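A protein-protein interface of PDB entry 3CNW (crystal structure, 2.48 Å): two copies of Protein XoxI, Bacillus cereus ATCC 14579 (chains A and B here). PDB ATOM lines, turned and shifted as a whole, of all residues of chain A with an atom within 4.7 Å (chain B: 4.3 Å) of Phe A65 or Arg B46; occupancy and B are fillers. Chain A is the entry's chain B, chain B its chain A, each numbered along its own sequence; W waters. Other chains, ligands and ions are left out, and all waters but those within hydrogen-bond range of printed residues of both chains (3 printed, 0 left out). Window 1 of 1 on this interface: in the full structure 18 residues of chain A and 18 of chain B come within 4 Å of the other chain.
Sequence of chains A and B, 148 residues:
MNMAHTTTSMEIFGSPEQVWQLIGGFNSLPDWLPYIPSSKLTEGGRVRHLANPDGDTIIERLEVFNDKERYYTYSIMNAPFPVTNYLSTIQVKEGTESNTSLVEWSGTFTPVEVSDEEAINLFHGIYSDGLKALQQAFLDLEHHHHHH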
ATOM      1  N   TRP A  20      18.393  26.074 -33.831  1.00  0.00           N
ATOM      2  CA  TRP A  20      19.675  26.076 -33.144  1.00  0.00           C
ATOM      3  C   TRP A  20      20.626  25.038 -33.702  1.00  0.00           C
ATOM      4  O   TRP A  20      21.837  25.236 -33.672  1.00  0.00           O
ATOM      5  CB  TRP A  20      19.481  25.851 -31.651  1.00  0.00           C
ATOM      6  CG  TRP A  20      20.763  25.607 -30.902  1.00  0.00           C
ATOM      7  CD1 TRP A  20      21.221  24.413 -30.445  1.00  0.00           C
ATOM      8  CD2 TRP A  20      21.721  26.594 -30.488  1.00  0.00           C
ATOM      9  NE1 TRP A  20      22.403  24.588 -29.761  1.00  0.00           N
ATOM     10  CE2 TRP A  20      22.734  25.915 -29.774  1.00  0.00           C
ATOM     11  CE3 TRP A  20      21.823  27.983 -30.656  1.00  0.00           C
ATOM     12  CZ2 TRP A  20      23.833  26.579 -29.215  1.00  0.00           C
ATOM     13  CZ3 TRP A  20      22.924  28.650 -30.098  1.00  0.00           C
ATOM     14  CH2 TRP A  20      23.912  27.940 -29.389  1.00  0.00           C
ATOM     15  N   GLN A  21      20.092  23.931 -34.211  1.00  0.00           N
ATOM     16  CA  GLN A  21      20.952  22.909 -34.787  1.00  0.00           C
ATOM     17  C   GLN A  21      21.688  23.459 -36.010  1.00  0.00           C
ATOM     18  O   GLN A  21      22.825  23.082 -36.279  1.00  0.00           O
ATOM     19  CB  GLN A  21      20.137  21.674 -35.177  1.00  0.00           C
ATOM     20  CG  GLN A  21      19.982  20.667 -34.039  1.00  0.00           C
ATOM     21  CD  GLN A  21      21.317  20.059 -33.594  1.00  0.00           C
ATOM     22  OE1 GLN A  21      21.948  19.318 -34.349  1.00  0.00           O
ATOM     23  NE2 GLN A  21      21.750  20.378 -32.372  1.00  0.00           N
ATOM     24  N   GLY A  24      23.829  26.981 -34.153  1.00  0.00           N
ATOM     25  CA  GLY A  24      24.588  26.904 -32.912  1.00  0.00           C
ATOM     26  C   GLY A  24      26.051  26.487 -33.010  1.00  0.00           C
ATOM     27  O   GLY A  24      26.751  26.446 -31.995  1.00  0.00           O
ATOM     28  N   GLY A  25      26.523  26.164 -34.210  1.00  0.00           N
ATOM     29  CA  GLY A  25      27.914  25.766 -34.356  1.00  0.00           C
ATOM     30  C   GLY A  25      28.784  27.003 -34.448  1.00  0.00           C
ATOM     31  O   GLY A  25      28.465  27.932 -35.195  1.00  0.00           O
ATOM     32  N   SER A  28      29.911  27.198 -37.892  1.00  0.00           N
ATOM     33  CA  SER A  28      28.855  27.013 -38.896  1.00  0.00           C
ATOM     34  C   SER A  28      28.303  28.264 -39.584  1.00  0.00           C
ATOM     35  O   SER A  28      27.262  28.186 -40.233  1.00  0.00           O
ATOM     36  CB  SER A  28      27.669  26.258 -38.288  1.00  0.00           C
ATOM     37  OG  SER A  28      28.055  24.982 -37.802  1.00  0.00           O
ATOM     38  N   LEU A  62      35.342  31.959 -28.712  1.00  0.00           N
ATOM     39  CA  LEU A  62      34.102  31.507 -28.097  1.00  0.00           C
ATOM     40  C   LEU A  62      34.243  31.813 -26.606  1.00  0.00           C
ATOM     41  O   LEU A  62      35.183  31.358 -25.956  1.00  0.00           O
ATOM     42  CB  LEU A  62      33.919  30.001 -28.307  1.00  0.00           C
ATOM     43  CG  LEU A  62      32.704  29.333 -27.655  1.00  0.00           C
ATOM     44  CD1 LEU A  62      31.397  29.903 -28.217  1.00  0.00           C
ATOM     45  CD2 LEU A  62      32.773  27.833 -27.907  1.00  0.00           C
ATOM     46  N   GLU A  63      33.310  32.587 -26.068  1.00  0.00           N
ATOM     47  CA  GLU A  63      33.364  32.948 -24.663  1.00  0.00           C
ATOM     48  C   GLU A  63      32.474  32.074 -23.798  1.00  0.00           C
ATOM     49  O   GLU A  63      32.878  31.632 -22.720  1.00  0.00           O
ATOM     50  CB  GLU A  63      32.966  34.416 -24.487  1.00  0.00           C
ATOM     51  CG  GLU A  63      33.977  35.406 -25.020  1.00  0.00           C
ATOM     52  CD  GLU A  63      35.309  35.287 -24.310  1.00  0.00           C
ATOM     53  OE1 GLU A  63      35.302  35.062 -23.081  1.00  0.00           O
ATOM     54  OE2 GLU A  63      36.365  35.427 -24.967  1.00  0.00           O
ATOM     55  N   VAL A  64      31.265  31.821 -24.279  1.00  0.00           N
ATOM     56  CA  VAL A  64      30.289  31.033 -23.550  1.00  0.00           C
ATOM     57  C   VAL A  64      29.471  30.244 -24.544  1.00  0.00           C
ATOM     58  O   VAL A  64      29.228  30.712 -25.657  1.00  0.00           O
ATOM     59  CB  VAL A  64      29.309  31.950 -22.770  1.00  0.00           C
ATOM     60  CG1 VAL A  64      28.278  31.101 -22.018  1.00  0.00           C
ATOM     61  CG2 VAL A  64      30.085  32.861 -21.810  1.00  0.00           C
ATOM     62  N   PHE A  65      29.041  29.057 -24.135  1.00  0.00           N
ATOM     63  CA  PHE A  65      28.215  28.198 -24.976  1.00  0.00           C
ATOM     64  C   PHE A  65      27.285  27.345 -24.129  1.00  0.00           C
ATOM     65  O   PHE A  65      27.712  26.697 -23.182  1.00  0.00           O
ATOM     66  CB  PHE A  65      29.086  27.275 -25.843  1.00  0.00           C
ATOM     67  CG  PHE A  65      28.301  26.247 -26.624  1.00  0.00           C
ATOM     68  CD1 PHE A  65      27.874  25.064 -26.030  1.00  0.00           C
ATOM     69  CD2 PHE A  65      28.006  26.459 -27.968  1.00  0.00           C
ATOM     70  CE1 PHE A  65      27.167  24.101 -26.766  1.00  0.00           C
ATOM     71  CE2 PHE A  65      27.301  25.506 -28.713  1.00  0.00           C
ATOM     72  CZ  PHE A  65      26.883  24.331 -28.114  1.00  0.00           C
ATOM     73  N   ASN A  66      26.008  27.347 -24.473  1.00  0.00           N
ATOM     74  CA  ASN A  66      25.050  26.529 -23.757  1.00  0.00           C
ATOM     75  C   ASN A  66      24.133  25.905 -24.802  1.00  0.00           C
ATOM     76  O   ASN A  66      23.418  26.597 -25.528  1.00  0.00           O
ATOM     77  CB  ASN A  66      24.252  27.365 -22.767  1.00  0.00           C
ATOM     78  CG  ASN A  66      23.382  26.510 -21.859  1.00  0.00           C
ATOM     79  OD1 ASN A  66      22.619  25.670 -22.333  1.00  0.00           O
ATOM     80  ND2 ASN A  66      23.483  26.726 -20.557  1.00  0.00           N
ATOM     81  N   ASP A  67      24.170  24.586 -24.890  1.00  0.00           N
ATOM     82  CA  ASP A  67      23.360  23.895 -25.869  1.00  0.00           C
ATOM     83  C   ASP A  67      21.859  24.017 -25.629  1.00  0.00           C
ATOM     84  O   ASP A  67      21.134  24.523 -26.476  1.00  0.00           O
ATOM     85  CB  ASP A  67      23.753  22.419 -25.930  1.00  0.00           C
ATOM     86  CG  ASP A  67      23.008  21.672 -27.013  1.00  0.00           C
ATOM     87  OD1 ASP A  67      23.254  21.943 -28.212  1.00  0.00           O
ATOM     88  OD2 ASP A  67      22.164  20.820 -26.660  1.00  0.00           O
ATOM     89  N   TYR A  71      22.397  29.240 -27.049  1.00  0.00           N
ATOM     90  CA  TYR A  71      23.050  30.521 -27.237  1.00  0.00           C
ATOM     91  C   TYR A  71      24.555  30.348 -27.126  1.00  0.00           C
ATOM     92  O   TYR A  71      25.039  29.340 -26.613  1.00  0.00           O
ATOM     93  CB  TYR A  71      22.556  31.552 -26.205  1.00  0.00           C
ATOM     94  CG  TYR A  71      23.109  31.390 -24.800  1.00  0.00           C
ATOM     95  CD1 TYR A  71      24.396  31.830 -24.465  1.00  0.00           C
ATOM     96  CD2 TYR A  71      22.331  30.827 -23.793  1.00  0.00           C
ATOM     97  CE1 TYR A  71      24.883  31.715 -23.152  1.00  0.00           C
ATOM     98  CE2 TYR A  71      22.804  30.709 -22.487  1.00  0.00           C
ATOM     99  CZ  TYR A  71      24.074  31.154 -22.172  1.00  0.00           C
ATOM    100  OH  TYR A  71      24.511  31.052 -20.869  1.00  0.00           O
ATOM    101  N   TYR A  72      25.289  31.327 -27.646  1.00  0.00           N
ATOM    102  CA  TYR A  72      26.738  31.317 -27.542  1.00  0.00           C
ATOM    103  C   TYR A  72      27.243  32.743 -27.675  1.00  0.00           C
ATOM    104  O   TYR A  72      26.777  33.515 -28.513  1.00  0.00           O
ATOM    105  CB  TYR A  72      27.386  30.358 -28.566  1.00  0.00           C
ATOM    106  CG  TYR A  72      27.479  30.806 -30.013  1.00  0.00           C
ATOM    107  CD1 TYR A  72      28.406  31.777 -30.425  1.00  0.00           C
ATOM    108  CD2 TYR A  72      26.709  30.180 -30.993  1.00  0.00           C
ATOM    109  CE1 TYR A  72      28.563  32.097 -31.794  1.00  0.00           C
ATOM    110  CE2 TYR A  72      26.855  30.488 -32.346  1.00  0.00           C
ATOM    111  CZ  TYR A  72      27.782  31.439 -32.746  1.00  0.00           C
ATOM    112  OH  TYR A  72      27.912  31.682 -34.098  1.00  0.00           O
ATOM    113  N   PHE B  26      37.419  21.538 -26.965  1.00  0.00           N
ATOM    114  CA  PHE B  26      36.576  20.362 -27.056  1.00  0.00           C
ATOM    115  C   PHE B  26      37.231  19.290 -27.940  1.00  0.00           C
ATOM    116  O   PHE B  26      36.934  18.105 -27.815  1.00  0.00           O
ATOM    117  CB  PHE B  26      35.191  20.736 -27.599  1.00  0.00           C
ATOM    118  CG  PHE B  26      34.141  19.664 -27.382  1.00  0.00           C
ATOM    119  CD1 PHE B  26      33.903  19.145 -26.106  1.00  0.00           C
ATOM    120  CD2 PHE B  26      33.392  19.170 -28.452  1.00  0.00           C
ATOM    121  CE1 PHE B  26      32.940  18.158 -25.900  1.00  0.00           C
ATOM    122  CE2 PHE B  26      32.425  18.181 -28.251  1.00  0.00           C
ATOM    123  CZ  PHE B  26      32.199  17.677 -26.973  1.00  0.00           C
ATOM    124  N   THR B  42      32.567  17.895 -35.423  1.00  0.00           N
ATOM    125  CA  THR B  42      31.532  18.022 -36.445  1.00  0.00           C
ATOM    126  C   THR B  42      30.470  18.946 -35.852  1.00  0.00           C
ATOM    127  O   THR B  42      30.595  19.381 -34.707  1.00  0.00           O
ATOM    128  CB  THR B  42      30.856  16.662 -36.813  1.00  0.00           C
ATOM    129  OG1 THR B  42      29.922  16.290 -35.794  1.00  0.00           O
ATOM    130  CG2 THR B  42      31.894  15.557 -36.969  1.00  0.00           C
ATOM    131  N   GLU B  43      29.437  19.262 -36.627  1.00  0.00           N
ATOM    132  CA  GLU B  43      28.370  20.122 -36.131  1.00  0.00           C
ATOM    133  C   GLU B  43      28.900  21.473 -35.680  1.00  0.00           C
ATOM    134  O   GLU B  43      28.532  21.979 -34.620  1.00  0.00           O
ATOM    135  CB  GLU B  43      27.650  19.435 -34.975  1.00  0.00           C
ATOM    136  CG  GLU B  43      26.696  18.343 -35.403  1.00  0.00           C
ATOM    137  CD  GLU B  43      25.310  18.889 -35.670  1.00  0.00           C
ATOM    138  OE1 GLU B  43      24.662  19.340 -34.696  1.00  0.00           O
ATOM    139  OE2 GLU B  43      24.878  18.881 -36.847  1.00  0.00           O
ATOM    140  N   GLY B  44      29.778  22.038 -36.496  1.00  0.00           N
ATOM    141  CA  GLY B  44      30.358  23.332 -36.205  1.00  0.00           C
ATOM    142  C   GLY B  44      31.178  23.393 -34.933  1.00  0.00           C
ATOM    143  O   GLY B  44      31.461  24.493 -34.447  1.00  0.00           O
ATOM    144  N   GLY B  45      31.549  22.233 -34.388  1.00  0.00           N
ATOM    145  CA  GLY B  45      32.348  22.205 -33.174  1.00  0.00           C
ATOM    146  C   GLY B  45      31.650  21.668 -31.933  1.00  0.00           C
ATOM    147  O   GLY B  45      32.288  21.424 -30.908  1.00  0.00           O
ATOM    148  N   ARG B  46      30.341  21.475 -32.014  1.00  0.00           N
ATOM    149  CA  ARG B  46      29.572  20.975 -30.884  1.00  0.00           C
ATOM    150  C   ARG B  46      29.721  19.478 -30.615  1.00  0.00           C
ATOM    151  O   ARG B  46      29.461  19.013 -29.504  1.00  0.00           O
ATOM    152  CB  ARG B  46      28.099  21.293 -31.094  1.00  0.00           C
ATOM    153  CG  ARG B  46      27.792  22.762 -31.001  1.00  0.00           C
ATOM    154  CD  ARG B  46      26.429  23.076 -31.557  1.00  0.00           C
ATOM    155  NE  ARG B  46      26.367  22.790 -32.985  1.00  0.00           N
ATOM    156  CZ  ARG B  46      25.311  23.044 -33.746  1.00  0.00           C
ATOM    157  NH1 ARG B  46      24.227  23.591 -33.206  1.00  0.00           N
ATOM    158  NH2 ARG B  46      25.343  22.757 -35.041  1.00  0.00           N
ATOM    159  N   VAL B  47      30.139  18.727 -31.622  1.00  0.00           N
ATOM    160  CA  VAL B  47      30.266  17.285 -31.472  1.00  0.00           C
ATOM    161  C   VAL B  47      31.664  16.781 -31.750  1.00  0.00           C
ATOM    162  O   VAL B  47      32.315  17.241 -32.688  1.00  0.00           O
ATOM    163  CB  VAL B  47      29.296  16.567 -32.430  1.00  0.00           C
ATOM    164  CG1 VAL B  47      29.527  15.053 -32.394  1.00  0.00           C
ATOM    165  CG2 VAL B  47      27.863  16.915 -32.055  1.00  0.00           C
ATOM    166  N   GLU B  60      30.628  12.495 -28.508  1.00  0.00           N
ATOM    167  CA  GLU B  60      30.111  13.300 -27.412  1.00  0.00           C
ATOM    168  C   GLU B  60      29.668  14.683 -27.869  1.00  0.00           C
ATOM    169  O   GLU B  60      30.131  15.201 -28.882  1.00  0.00           O
ATOM    170  CB  GLU B  60      31.176  13.425 -26.315  1.00  0.00           C
ATOM    171  CG  GLU B  60      31.794  12.100 -25.900  1.00  0.00           C
ATOM    172  CD  GLU B  60      32.879  12.260 -24.846  1.00  0.00           C
ATOM    173  OE1 GLU B  60      33.622  13.273 -24.892  1.00  0.00           O
ATOM    174  OE2 GLU B  60      32.997  11.361 -23.981  1.00  0.00           O
ATOM    175  N   ARG B  61      28.771  15.284 -27.105  1.00  0.00           N
ATOM    176  CA  ARG B  61      28.262  16.592 -27.447  1.00  0.00           C
ATOM    177  C   ARG B  61      28.546  17.622 -26.366  1.00  0.00           C
ATOM    178  O   ARG B  61      28.396  17.347 -25.173  1.00  0.00           O
ATOM    179  CB  ARG B  61      26.754  16.508 -27.704  1.00  0.00           C
ATOM    180  CG  ARG B  61      25.996  17.792 -27.423  1.00  0.00           C
ATOM    181  CD  ARG B  61      24.636  17.763 -28.073  1.00  0.00           C
ATOM    182  NE  ARG B  61      24.729  18.154 -29.475  1.00  0.00           N
ATOM    183  CZ  ARG B  61      24.224  17.455 -30.481  1.00  0.00           C
ATOM    184  NH1 ARG B  61      23.586  16.317 -30.248  1.00  0.00           N
ATOM    185  NH2 ARG B  61      24.350  17.902 -31.719  1.00  0.00           N
ATOM    186  N   LEU B  62      28.963  18.809 -26.794  1.00  0.00           N
ATOM    187  CA  LEU B  62      29.243  19.897 -25.871  1.00  0.00           C
ATOM    188  C   LEU B  62      27.905  20.441 -25.370  1.00  0.00           C
ATOM    189  O   LEU B  62      27.030  20.771 -26.168  1.00  0.00           O
ATOM    190  CB  LEU B  62      30.022  21.004 -26.590  1.00  0.00           C
ATOM    191  CG  LEU B  62      30.296  22.279 -25.789  1.00  0.00           C
ATOM    192  CD1 LEU B  62      31.218  21.962 -24.616  1.00  0.00           C
ATOM    193  CD2 LEU B  62      30.916  23.315 -26.693  1.00  0.00           C
ATOM    194  N   GLU B  63      27.747  20.529 -24.053  1.00  0.00           N
ATOM    195  CA  GLU B  63      26.512  21.027 -23.458  1.00  0.00           C
ATOM    196  C   GLU B  63      26.726  22.449 -22.947  1.00  0.00           C
ATOM    197  O   GLU B  63      25.901  23.334 -23.176  1.00  0.00           O
ATOM    198  CB  GLU B  63      26.088  20.131 -22.288  1.00  0.00           C
ATOM    199  CG  GLU B  63      25.692  18.699 -22.641  1.00  0.00           C
ATOM    200  CD  GLU B  63      24.345  18.608 -23.346  1.00  0.00           C
ATOM    201  OE1 GLU B  63      23.528  19.546 -23.215  1.00  0.00           O
ATOM    202  OE2 GLU B  63      24.099  17.585 -24.022  1.00  0.00           O
ATOM    203  N   VAL B  64      27.848  22.658 -22.256  1.00  0.00           N
ATOM    204  CA  VAL B  64      28.186  23.961 -21.683  1.00  0.00           C
ATOM    205  C   VAL B  64      29.689  24.272 -21.758  1.00  0.00           C
ATOM    206  O   VAL B  64      30.530  23.408 -21.527  1.00  0.00           O
ATOM    207  CB  VAL B  64      27.749  24.037 -20.185  1.00  0.00           C
ATOM    208  CG1 VAL B  64      27.986  25.447 -19.632  1.00  0.00           C
ATOM    209  CG2 VAL B  64      26.290  23.644 -20.043  1.00  0.00           C
ATOM    210  N   PHE B  65      30.011  25.521 -22.070  1.00  0.00           N
ATOM    211  CA  PHE B  65      31.388  25.958 -22.151  1.00  0.00           C
ATOM    212  C   PHE B  65      31.508  27.387 -21.679  1.00  0.00           C
ATOM    213  O   PHE B  65      30.756  28.256 -22.101  1.00  0.00           O
ATOM    214  CB  PHE B  65      31.915  25.859 -23.588  1.00  0.00           C
ATOM    215  CG  PHE B  65      33.273  26.492 -23.789  1.00  0.00           C
ATOM    216  CD1 PHE B  65      33.402  27.866 -24.006  1.00  0.00           C
ATOM    217  CD2 PHE B  65      34.426  25.705 -23.766  1.00  0.00           C
ATOM    218  CE1 PHE B  65      34.676  28.456 -24.206  1.00  0.00           C
ATOM    219  CE2 PHE B  65      35.695  26.274 -23.961  1.00  0.00           C
ATOM    220  CZ  PHE B  65      35.819  27.664 -24.184  1.00  0.00           C
HETATM  221  O   HOH W   1      23.454  22.234 -22.679  1.00  0.00           O
HETATM  222  O   HOH W   2      26.626  22.979 -37.523  1.00  0.00           O
HETATM  223  O   HOH W   3      26.046  20.810 -28.748  1.00  0.00           O
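The side-chain carboxylate (OE1) of Glu B43 lies close to the side-chain amide oxygen (OE1) of Gln A21.
The guanidinium group (NH1) of Arg B46 lies within hydrogen-bond range of the backbone carbonyl oxygen (O) of Trp A20 (2.9 Å).
The backbone carbonyl oxygen (O) of Gln A21 sits at hydrogen-bond distance from the guanidinium group (NH2) of Arg B46 (2.8 Å).
The backbone carbonyl oxygen of Glu B63 is in hydrogen-bond range of the backbone NH of Asp A67, at 2.7 Å.
O of Phe B65 is in hydrogen-bond range of N of Phe A65.
OE1 of Glu B43 is in salt-bridge range of NH2 of Arg B46, at 3.5 Å.
The guanidinium group of Arg B61 lies within salt-bridge range of the side-chain carboxylate of Glu B43 (3.3 Å).
The backbone carbonyl oxygen (O) of Arg B46 lies within hydrogen-bond range of the backbone NH (N) of Leu B62 (2.8 Å).
The indole nitrogen (NE1) of Trp A20 is in hydrogen-bond range of the side-chain carboxylate (OD1) of Asp A67 (3.2 Å).
The backbone carbonyl oxygen of Tyr A71 sits at hydrogen-bond distance from the backbone NH of Asn A66 (3.1 Å).
Among the printed residues, pairs that only touch across the chains: Gln A21 with Arg B61 (3.6 Å), Gly A24 with Arg B46 (3.3 Å), Gly A25 with Glu B43 (3.8 Å), Gly A25 with Gly B44 (3.7 Å), Gly A25 with Arg B46 (3.4 Å), Ser A28 with Gly B44 (3.3 Å), Leu A62 with Phe B65 (3.4 Å), Glu A63 with Phe B65 (3.9 Å), Val A64 with Phe B65 (3.2 Å), Phe A65 with Arg B46 (3.4 Å), Phe A65 with Leu B62 (3.4 Å), Phe A65 with Glu B63 (3.8 Å), Phe A65 with Val B64 (3.2 Å), Asn A66 with Glu B63 (3.4 Å) and Asp A67 with Leu B62 (3.7 Å).
Of the printed residues of chain B, Phe A65 touches Arg B46 (3.4 Å), Leu B62 (3.4 Å), Glu B63 (3.8 Å), Val B64 (3.2 Å) and Phe B65 (2.8 Å).
Arg B46 touches just these residues of chain A: Trp A20, Gln A21, Gly A24, Gly A25 and Phe A65.
Of the printed residues of chain B, Gln A21 touches Glu B43, Arg B46 and Arg B61.
Of the printed residues of chain A, Arg B61 touches Gln A21.
Tyr A72 touches none of the printed residues of chain B.
Val B47 touches none of the printed residues of chain A.
The nearest printed residue of chain B that does not touch Phe A65 is Arg B61 (6.5 Å).
Printed residues of chain B that touch a printed residue of chain A: Glu B43, Gly B44, Arg B46, Arg B61, Leu B62, Glu B63, Val B64 and Phe B65.
Hydrophobic or aromatic side chains of chain B within 4 Å of the printed part of chain A: Leu B62, Val B64 and Phe B65.
Along chain B the printed residues that touch a printed residue of chain A span positions 43 to 65.
Of the 13 printed residues of chain A, 11 touch a printed residue of chain B.
Printed residues of chain A that touch a printed residue of chain B: Trp A20, Gln A21, Gly A24, Gly A25, Ser A28, Leu A62, Glu A63, Val A64, Phe A65, Asn A66 and Asp A67.
Among the printed residues, no Asp or Glu carboxylate lies within 4 Å of a Lys or Arg side-chain nitrogen of the other chain.
Leu A62 touches Phe B65, and with the chains exchanged Phe A65 touches Leu B62.
Glu A63 touches Phe B65, and with the chains exchanged Phe A65 touches Glu B63.
Val A64 touches Phe B65, and with the chains exchanged Phe A65 touches Val B64.
Phe B65 touches its own counterpart, Phe A65.
Of the 20 pairs that touch across the chains among the printed residues, 7 have their exchanged pair printed and touching as well.
Water W2 lies within hydrogen-bond range of the side-chain hydroxyl (OG) of Ser A28 (2.5 Å), the guanidinium group (NH2) of Arg B46 (2.8 Å) and the backbone NH (N) of Gly B44 (3.4 Å).
Water W1 lies within hydrogen-bond range of O of Glu B63 (2.7 Å) and N of Asp A67 (3.3 Å).
Water W3 lies within hydrogen-bond range of O of Leu B62 (2.8 Å), NE of Arg B61 (3.1 Å) and OD1 of Asp A67 (3.1 Å).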
